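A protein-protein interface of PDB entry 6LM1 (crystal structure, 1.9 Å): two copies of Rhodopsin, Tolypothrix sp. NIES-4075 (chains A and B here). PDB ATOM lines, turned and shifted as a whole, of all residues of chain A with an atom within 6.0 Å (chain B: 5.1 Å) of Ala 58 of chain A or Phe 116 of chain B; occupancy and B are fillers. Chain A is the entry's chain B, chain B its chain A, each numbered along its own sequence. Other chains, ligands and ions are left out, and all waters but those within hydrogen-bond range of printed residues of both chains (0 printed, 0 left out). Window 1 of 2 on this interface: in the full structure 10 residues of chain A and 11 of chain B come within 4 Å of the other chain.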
ATOM      1  N   PHE A  20      -8.668  10.444  -0.277  1.00  0.00           N
ATOM      2  CA  PHE A  20      -9.964  10.918   0.192  1.00  0.00           C
ATOM      3  C   PHE A  20     -10.744   9.796   0.864  1.00  0.00           C
ATOM      4  O   PHE A  20     -11.300   9.974   1.956  1.00  0.00           O
ATOM      5  CB  PHE A  20     -10.764  11.493  -0.980  1.00  0.00           C
ATOM      6  CG  PHE A  20     -12.160  11.909  -0.612  1.00  0.00           C
ATOM      7  CD1 PHE A  20     -12.369  12.920   0.316  1.00  0.00           C
ATOM      8  CD2 PHE A  20     -13.256  11.295  -1.193  1.00  0.00           C
ATOM      9  CE1 PHE A  20     -13.658  13.305   0.658  1.00  0.00           C
ATOM     10  CE2 PHE A  20     -14.543  11.678  -0.857  1.00  0.00           C
ATOM     11  CZ  PHE A  20     -14.732  12.702   0.074  1.00  0.00           C
ATOM     12  N   MET A  23      -9.341   8.811   4.231  1.00  0.00           N
ATOM     13  CA  MET A  23      -9.666   9.748   5.306  1.00  0.00           C
ATOM     14  C   MET A  23     -11.129   9.636   5.726  1.00  0.00           C
ATOM     15  O   MET A  23     -11.444   9.757   6.917  1.00  0.00           O
ATOM     16  CB  MET A  23      -9.330  11.181   4.881  1.00  0.00           C
ATOM     17  CG  MET A  23      -7.847  11.421   4.585  1.00  0.00           C
ATOM     18  SD  MET A  23      -6.716  11.005   5.923  1.00  0.00           S
ATOM     19  CE  MET A  23      -5.131  11.107   5.085  1.00  0.00           C
ATOM     20  N   VAL A  53      -8.354  13.648  10.393  1.00  0.00           N
ATOM     21  CA  VAL A  53      -8.754  13.034   9.129  1.00  0.00           C
ATOM     22  C   VAL A  53      -9.915  13.799   8.490  1.00  0.00           C
ATOM     23  O   VAL A  53     -10.088  13.753   7.268  1.00  0.00           O
ATOM     24  CB  VAL A  53      -9.098  11.540   9.316  1.00  0.00           C
ATOM     25  CG1 VAL A  53      -7.855  10.747   9.684  1.00  0.00           C
ATOM     26  CG2 VAL A  53     -10.190  11.346  10.365  1.00  0.00           C
ATOM     27  N   LEU A  54     -10.723  14.505   9.284  1.00  0.00           N
ATOM     28  CA  LEU A  54     -11.748  15.367   8.702  1.00  0.00           C
ATOM     29  C   LEU A  54     -11.118  16.469   7.857  1.00  0.00           C
ATOM     30  O   LEU A  54     -11.517  16.709   6.711  1.00  0.00           O
ATOM     31  CB  LEU A  54     -12.612  15.987   9.804  1.00  0.00           C
ATOM     32  CG  LEU A  54     -13.670  16.955   9.265  1.00  0.00           C
ATOM     33  CD1 LEU A  54     -14.870  16.169   8.721  1.00  0.00           C
ATOM     34  CD2 LEU A  54     -14.113  17.961  10.320  1.00  0.00           C
ATOM     35  N   TRP A  55     -10.122  17.154   8.410  1.00  0.00           N
ATOM     36  CA  TRP A  55      -9.482  18.228   7.666  1.00  0.00           C
ATOM     37  C   TRP A  55      -8.755  17.687   6.437  1.00  0.00           C
ATOM     38  O   TRP A  55      -8.898  18.228   5.336  1.00  0.00           O
ATOM     39  CB  TRP A  55      -8.528  18.985   8.590  1.00  0.00           C
ATOM     40  CG  TRP A  55      -7.950  20.209   7.968  1.00  0.00           C
ATOM     41  CD1 TRP A  55      -6.660  20.381   7.538  1.00  0.00           C
ATOM     42  CD2 TRP A  55      -8.631  21.445   7.708  1.00  0.00           C
ATOM     43  NE1 TRP A  55      -6.497  21.649   7.026  1.00  0.00           N
ATOM     44  CE2 TRP A  55      -7.691  22.323   7.118  1.00  0.00           C
ATOM     45  CE3 TRP A  55      -9.943  21.893   7.904  1.00  0.00           C
ATOM     46  CZ2 TRP A  55      -8.024  23.619   6.724  1.00  0.00           C
ATOM     47  CZ3 TRP A  55     -10.269  23.186   7.521  1.00  0.00           C
ATOM     48  CH2 TRP A  55      -9.310  24.036   6.940  1.00  0.00           C
ATOM     49  N   ALA A  56      -7.984  16.604   6.598  1.00  0.00           N
ATOM     50  CA  ALA A  56      -7.275  16.021   5.458  1.00  0.00           C
ATOM     51  C   ALA A  56      -8.246  15.531   4.383  1.00  0.00           C
ATOM     52  O   ALA A  56      -7.999  15.709   3.182  1.00  0.00           O
ATOM     53  CB  ALA A  56      -6.373  14.872   5.923  1.00  0.00           C
ATOM     54  N   GLY A  57      -9.348  14.898   4.789  1.00  0.00           N
ATOM     55  CA  GLY A  57     -10.328  14.450   3.808  1.00  0.00           C
ATOM     56  C   GLY A  57     -10.967  15.603   3.056  1.00  0.00           C
ATOM     57  O   GLY A  57     -11.152  15.535   1.840  1.00  0.00           O
ATOM     58  N   ALA A  58     -11.296  16.688   3.767  1.00  0.00           N
ATOM     59  CA  ALA A  58     -11.859  17.858   3.099  1.00  0.00           C
ATOM     60  C   ALA A  58     -10.868  18.441   2.098  1.00  0.00           C
ATOM     61  O   ALA A  58     -11.251  18.825   0.988  1.00  0.00           O
ATOM     62  CB  ALA A  58     -12.270  18.922   4.133  1.00  0.00           C
ATOM     63  N   LEU A  59      -9.586  18.537   2.474  1.00  0.00           N
ATOM     64  CA  LEU A  59      -8.607  19.079   1.534  1.00  0.00           C
ATOM     65  C   LEU A  59      -8.369  18.129   0.359  1.00  0.00           C
ATOM     66  O   LEU A  59      -8.163  18.578  -0.777  1.00  0.00           O
ATOM     67  CB  LEU A  59      -7.294  19.397   2.258  1.00  0.00           C
ATOM     68  CG  LEU A  59      -7.192  20.848   2.757  1.00  0.00           C
ATOM     69  CD1 LEU A  59      -7.241  21.814   1.569  1.00  0.00           C
ATOM     70  CD2 LEU A  59      -8.289  21.194   3.770  1.00  0.00           C
ATOM     71  N   TYR A  60      -8.390  16.813   0.597  1.00  0.00           N
ATOM     72  CA  TYR A  60      -8.339  15.891  -0.538  1.00  0.00           C
ATOM     73  C   TYR A  60      -9.521  16.125  -1.478  1.00  0.00           C
ATOM     74  O   TYR A  60      -9.354  16.155  -2.702  1.00  0.00           O
ATOM     75  CB  TYR A  60      -8.294  14.438  -0.055  1.00  0.00           C
ATOM     76  CG  TYR A  60      -6.880  13.889   0.014  1.00  0.00           C
ATOM     77  CD1 TYR A  60      -6.232  13.457  -1.132  1.00  0.00           C
ATOM     78  CD2 TYR A  60      -6.187  13.835   1.224  1.00  0.00           C
ATOM     79  CE1 TYR A  60      -4.925  12.963  -1.081  1.00  0.00           C
ATOM     80  CE2 TYR A  60      -4.887  13.336   1.288  1.00  0.00           C
ATOM     81  CZ  TYR A  60      -4.264  12.904   0.129  1.00  0.00           C
ATOM     82  OH  TYR A  60      -2.969  12.417   0.173  1.00  0.00           O
ATOM     83  N   LEU A  61     -10.715  16.327  -0.925  1.00  0.00           N
ATOM     84  CA  LEU A  61     -11.863  16.655  -1.767  1.00  0.00           C
ATOM     85  C   LEU A  61     -11.637  17.953  -2.550  1.00  0.00           C
ATOM     86  O   LEU A  61     -11.995  18.033  -3.729  1.00  0.00           O
ATOM     87  CB  LEU A  61     -13.133  16.734  -0.914  1.00  0.00           C
ATOM     88  CG  LEU A  61     -14.457  16.921  -1.659  1.00  0.00           C
ATOM     89  CD1 LEU A  61     -14.665  15.828  -2.723  1.00  0.00           C
ATOM     90  CD2 LEU A  61     -15.618  16.936  -0.667  1.00  0.00           C
ATOM     91  N   THR A  62     -11.042  18.983  -1.926  1.00  0.00           N
ATOM     92  CA  THR A  62     -10.798  20.211  -2.696  1.00  0.00           C
ATOM     93  C   THR A  62      -9.830  19.966  -3.851  1.00  0.00           C
ATOM     94  O   THR A  62      -9.922  20.637  -4.884  1.00  0.00           O
ATOM     95  CB  THR A  62     -10.262  21.355  -1.813  1.00  0.00           C
ATOM     96  OG1 THR A  62      -8.971  21.009  -1.311  1.00  0.00           O
ATOM     97  CG2 THR A  62     -11.201  21.648  -0.654  1.00  0.00           C
ATOM     98  N   MET A  63      -8.908  19.012  -3.711  1.00  0.00           N
ATOM     99  CA  MET A  63      -7.999  18.715  -4.815  1.00  0.00           C
ATOM    100  C   MET A  63      -8.682  17.882  -5.903  1.00  0.00           C
ATOM    101  O   MET A  63      -8.470  18.125  -7.098  1.00  0.00           O
ATOM    102  CB  MET A  63      -6.746  18.019  -4.280  1.00  0.00           C
ATOM    103  CG  MET A  63      -5.866  18.985  -3.465  1.00  0.00           C
ATOM    104  SD  MET A  63      -4.219  18.367  -3.059  1.00  0.00           S
ATOM    105  CE  MET A  63      -4.590  17.166  -1.777  1.00  0.00           C
ATOM    106  N   ILE B 111     -15.056  25.100  18.549  1.00  0.00           N
ATOM    107  CA  ILE B 111     -14.494  26.193  17.756  1.00  0.00           C
ATOM    108  C   ILE B 111     -13.895  25.658  16.456  1.00  0.00           C
ATOM    109  O   ILE B 111     -14.076  26.254  15.385  1.00  0.00           O
ATOM    110  CB  ILE B 111     -13.463  26.977  18.591  1.00  0.00           C
ATOM    111  CG1 ILE B 111     -14.188  27.910  19.563  1.00  0.00           C
ATOM    112  CG2 ILE B 111     -12.516  27.771  17.686  1.00  0.00           C
ATOM    113  CD1 ILE B 111     -13.271  28.656  20.520  1.00  0.00           C
ATOM    114  N   ALA B 112     -13.206  24.513  16.520  1.00  0.00           N
ATOM    115  CA  ALA B 112     -12.691  23.887  15.300  1.00  0.00           C
ATOM    116  C   ALA B 112     -13.822  23.534  14.335  1.00  0.00           C
ATOM    117  O   ALA B 112     -13.715  23.782  13.131  1.00  0.00           O
ATOM    118  CB  ALA B 112     -11.885  22.633  15.647  1.00  0.00           C
ATOM    119  N   ALA B 113     -14.916  22.949  14.847  1.00  0.00           N
ATOM    120  CA  ALA B 113     -16.070  22.672  13.992  1.00  0.00           C
ATOM    121  C   ALA B 113     -16.620  23.948  13.366  1.00  0.00           C
ATOM    122  O   ALA B 113     -17.039  23.952  12.200  1.00  0.00           O
ATOM    123  CB  ALA B 113     -17.164  21.967  14.800  1.00  0.00           C
ATOM    124  N   ASP B 114     -16.653  25.039  14.140  1.00  0.00           N
ATOM    125  CA  ASP B 114     -17.202  26.290  13.635  1.00  0.00           C
ATOM    126  C   ASP B 114     -16.323  26.894  12.544  1.00  0.00           C
ATOM    127  O   ASP B 114     -16.837  27.407  11.537  1.00  0.00           O
ATOM    128  CB  ASP B 114     -17.378  27.272  14.798  1.00  0.00           C
ATOM    129  CG  ASP B 114     -17.866  28.613  14.342  1.00  0.00           C
ATOM    130  OD1 ASP B 114     -19.090  28.810  14.295  1.00  0.00           O
ATOM    131  OD2 ASP B 114     -17.030  29.465  13.994  1.00  0.00           O
ATOM    132  N   ILE B 115     -15.001  26.876  12.733  1.00  0.00           N
ATOM    133  CA  ILE B 115     -14.111  27.360  11.675  1.00  0.00           C
ATOM    134  C   ILE B 115     -14.271  26.508  10.419  1.00  0.00           C
ATOM    135  O   ILE B 115     -14.329  27.028   9.296  1.00  0.00           O
ATOM    136  CB  ILE B 115     -12.650  27.391  12.168  1.00  0.00           C
ATOM    137  CG1 ILE B 115     -12.476  28.485  13.231  1.00  0.00           C
ATOM    138  CG2 ILE B 115     -11.703  27.693  10.990  1.00  0.00           C
ATOM    139  CD1 ILE B 115     -11.186  28.339  14.064  1.00  0.00           C
ATOM    140  N   PHE B 116     -14.379  25.186  10.592  1.00  0.00           N
ATOM    141  CA  PHE B 116     -14.637  24.297   9.457  1.00  0.00           C
ATOM    142  C   PHE B 116     -15.955  24.649   8.769  1.00  0.00           C
ATOM    143  O   PHE B 116     -16.036  24.671   7.535  1.00  0.00           O
ATOM    144  CB  PHE B 116     -14.639  22.843   9.950  1.00  0.00           C
ATOM    145  CG  PHE B 116     -14.887  21.815   8.875  1.00  0.00           C
ATOM    146  CD1 PHE B 116     -13.825  21.296   8.129  1.00  0.00           C
ATOM    147  CD2 PHE B 116     -16.175  21.349   8.622  1.00  0.00           C
ATOM    148  CE1 PHE B 116     -14.047  20.328   7.151  1.00  0.00           C
ATOM    149  CE2 PHE B 116     -16.408  20.381   7.640  1.00  0.00           C
ATOM    150  CZ  PHE B 116     -15.340  19.876   6.904  1.00  0.00           C
ATOM    151  N   MET B 117     -17.000  24.933   9.553  1.00  0.00           N
ATOM    152  CA  MET B 117     -18.287  25.339   8.979  1.00  0.00           C
ATOM    153  C   MET B 117     -18.155  26.598   8.124  1.00  0.00           C
ATOM    154  O   MET B 117     -18.702  26.675   7.019  1.00  0.00           O
ATOM    155  CB  MET B 117     -19.307  25.567  10.102  1.00  0.00           C
ATOM    156  CG  MET B 117     -20.647  26.168   9.625  1.00  0.00           C
ATOM    157  SD  MET B 117     -21.751  26.524  11.005  1.00  0.00           S
ATOM    158  CE  MET B 117     -21.014  28.032  11.691  1.00  0.00           C
ATOM    159  N   ILE B 118     -17.479  27.624   8.647  1.00  0.00           N
ATOM    160  CA  ILE B 118     -17.352  28.876   7.895  1.00  0.00           C
ATOM    161  C   ILE B 118     -16.500  28.666   6.643  1.00  0.00           C
ATOM    162  O   ILE B 118     -16.824  29.173   5.563  1.00  0.00           O
ATOM    163  CB  ILE B 118     -16.775  29.985   8.805  1.00  0.00           C
ATOM    164  CG1 ILE B 118     -17.717  30.261   9.995  1.00  0.00           C
ATOM    165  CG2 ILE B 118     -16.495  31.275   8.008  1.00  0.00           C
ATOM    166  CD1 ILE B 118     -19.170  30.620   9.607  1.00  0.00           C
ATOM    167  N   LEU B 119     -15.393  27.928   6.763  1.00  0.00           N
ATOM    168  CA  LEU B 119     -14.494  27.790   5.619  1.00  0.00           C
ATOM    169  C   LEU B 119     -15.123  26.939   4.515  1.00  0.00           C
ATOM    170  O   LEU B 119     -14.930  27.213   3.328  1.00  0.00           O
ATOM    171  CB  LEU B 119     -13.151  27.193   6.065  1.00  0.00           C
ATOM    172  CG  LEU B 119     -12.311  28.121   6.956  1.00  0.00           C
ATOM    173  CD1 LEU B 119     -10.977  27.458   7.344  1.00  0.00           C
ATOM    174  CD2 LEU B 119     -12.074  29.449   6.236  1.00  0.00           C
ATOM    175  N   THR B 120     -15.858  25.888   4.876  1.00  0.00           N
ATOM    176  CA  THR B 120     -16.557  25.144   3.830  1.00  0.00           C
ATOM    177  C   THR B 120     -17.687  25.975   3.228  1.00  0.00           C
ATOM    178  O   THR B 120     -18.002  25.827   2.037  1.00  0.00           O
ATOM    179  CB  THR B 120     -17.082  23.801   4.366  1.00  0.00           C
ATOM    180  OG1 THR B 120     -17.853  23.997   5.559  1.00  0.00           O
ATOM    181  CG2 THR B 120     -15.897  22.863   4.688  1.00  0.00           C
ATOM    182  N   GLY B 121     -18.287  26.871   4.015  1.00  0.00           N
ATOM    183  CA  GLY B 121     -19.260  27.792   3.444  1.00  0.00           C
ATOM    184  C   GLY B 121     -18.620  28.765   2.470  1.00  0.00           C
ATOM    185  O   GLY B 121     -19.211  29.125   1.449  1.00  0.00           O
ATOM    186  N   TRP B 135     -20.586  21.468  -0.919  1.00  0.00           N
ATOM    187  CA  TRP B 135     -19.941  22.120   0.217  1.00  0.00           C
ATOM    188  C   TRP B 135     -20.961  22.717   1.177  1.00  0.00           C
ATOM    189  O   TRP B 135     -20.716  22.763   2.389  1.00  0.00           O
ATOM    190  CB  TRP B 135     -18.980  23.190  -0.285  1.00  0.00           C
ATOM    191  CG  TRP B 135     -17.768  22.573  -0.907  1.00  0.00           C
ATOM    192  CD1 TRP B 135     -17.446  22.540  -2.229  1.00  0.00           C
ATOM    193  CD2 TRP B 135     -16.739  21.855  -0.221  1.00  0.00           C
ATOM    194  NE1 TRP B 135     -16.256  21.865  -2.412  1.00  0.00           N
ATOM    195  CE2 TRP B 135     -15.810  21.426  -1.189  1.00  0.00           C
ATOM    196  CE3 TRP B 135     -16.515  21.534   1.127  1.00  0.00           C
ATOM    197  CZ2 TRP B 135     -14.662  20.698  -0.857  1.00  0.00           C
ATOM    198  CZ3 TRP B 135     -15.373  20.809   1.456  1.00  0.00           C
ATOM    199  CH2 TRP B 135     -14.463  20.402   0.464  1.00  0.00           C
ATOM    200  N   ILE B 138     -21.985  19.850   3.392  1.00  0.00           N
ATOM    201  CA  ILE B 138     -20.895  19.556   4.326  1.00  0.00           C
ATOM    202  C   ILE B 138     -20.855  20.597   5.447  1.00  0.00           C
ATOM    203  O   ILE B 138     -20.711  20.262   6.628  1.00  0.00           O
ATOM    204  CB  ILE B 138     -19.553  19.491   3.572  1.00  0.00           C
ATOM    205  CG1 ILE B 138     -19.466  18.217   2.717  1.00  0.00           C
ATOM    206  CG2 ILE B 138     -18.381  19.551   4.534  1.00  0.00           C
ATOM    207  CD1 ILE B 138     -18.392  18.284   1.630  1.00  0.00           C
ATOM    208  N   ALA B 142     -21.459  20.262   9.718  1.00  0.00           N
ATOM    209  CA  ALA B 142     -20.722  20.862  10.823  1.00  0.00           C
ATOM    210  C   ALA B 142     -21.643  21.705  11.710  1.00  0.00           C
ATOM    211  O   ALA B 142     -21.529  21.674  12.937  1.00  0.00           O
ATOM    212  CB  ALA B 142     -19.567  21.706  10.273  1.00  0.00           C
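Among the printed residues, pairs that only touch across the chains: Thr 62 of chain A with Trp 135 of chain B (3.6 Å), Ala 58 of chain A with Trp 135 of chain B (3.6 Å), Ala 58 of chain A with Phe 116 of chain B (3.8 Å), Leu 61 of chain A with Trp 135 of chain B (3.8 Å), Trp 55 of chain A with Leu 119 of chain B (3.8 Å), Leu 61 of chain A with Ile 138 of chain B (3.8 Å), Trp 55 of chain A with Phe 116 of chain B (3.9 Å) and Leu 54 of chain A with Phe 116 of chain B (3.96 Å).
Of the 14 printed residues of chain B, 4 touch a printed residue of chain A. Printed residues of chain B that touch a printed residue of chain A: Phe 116, Leu 119, Trp 135 and Ile 138. Hydrophobic or aromatic side chains of chain B that line the printed part of chain A: Phe 116, Leu 119, Trp 135 and Ile 138.
No position is printed for both chains. Of the 8 pairs that touch across the chains among the printed residues, none has its exchanged pair printed and touching as well.
The side-chain hydroxyl of Thr 62 of chain A is in hydrogen-bond range of the backbone carbonyl oxygen of Leu 59 of chain A (2.6 Å). O of Phe 116 of chain B is in hydrogen-bond range of OG1 of Thr 120 of chain B (2.8 Å).
Ala 58 of chain A touches two residues of chain B. Of the printed residues of chain B, Thr 62 of chain A touches Trp 135. Phe 116 of chain B touches just these residues of chain A: Leu 54 (3.96 Å), Trp 55 (3.9 Å) and Ala 58 (3.8 Å). Thr 120 of chain B touches none of the printed residues of chain A. Of the printed residues of chain A, Trp 135 of chain B touches Ala 58, Leu 61 and Thr 62. Ala 142 of chain B touches none of the printed residues of chain A. The nearest printed residue of chain B that does not touch Ala 58 of chain A is Thr 120 of chain B (5.4 Å). The nearest printed residue of chain A that does not touch Phe 116 of chain B is Leu 59 of chain A (6.7 Å). The nearest printed residue of chain A that does not touch Ile 138 of chain B is Ala 58 of chain A (6.2 Å).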
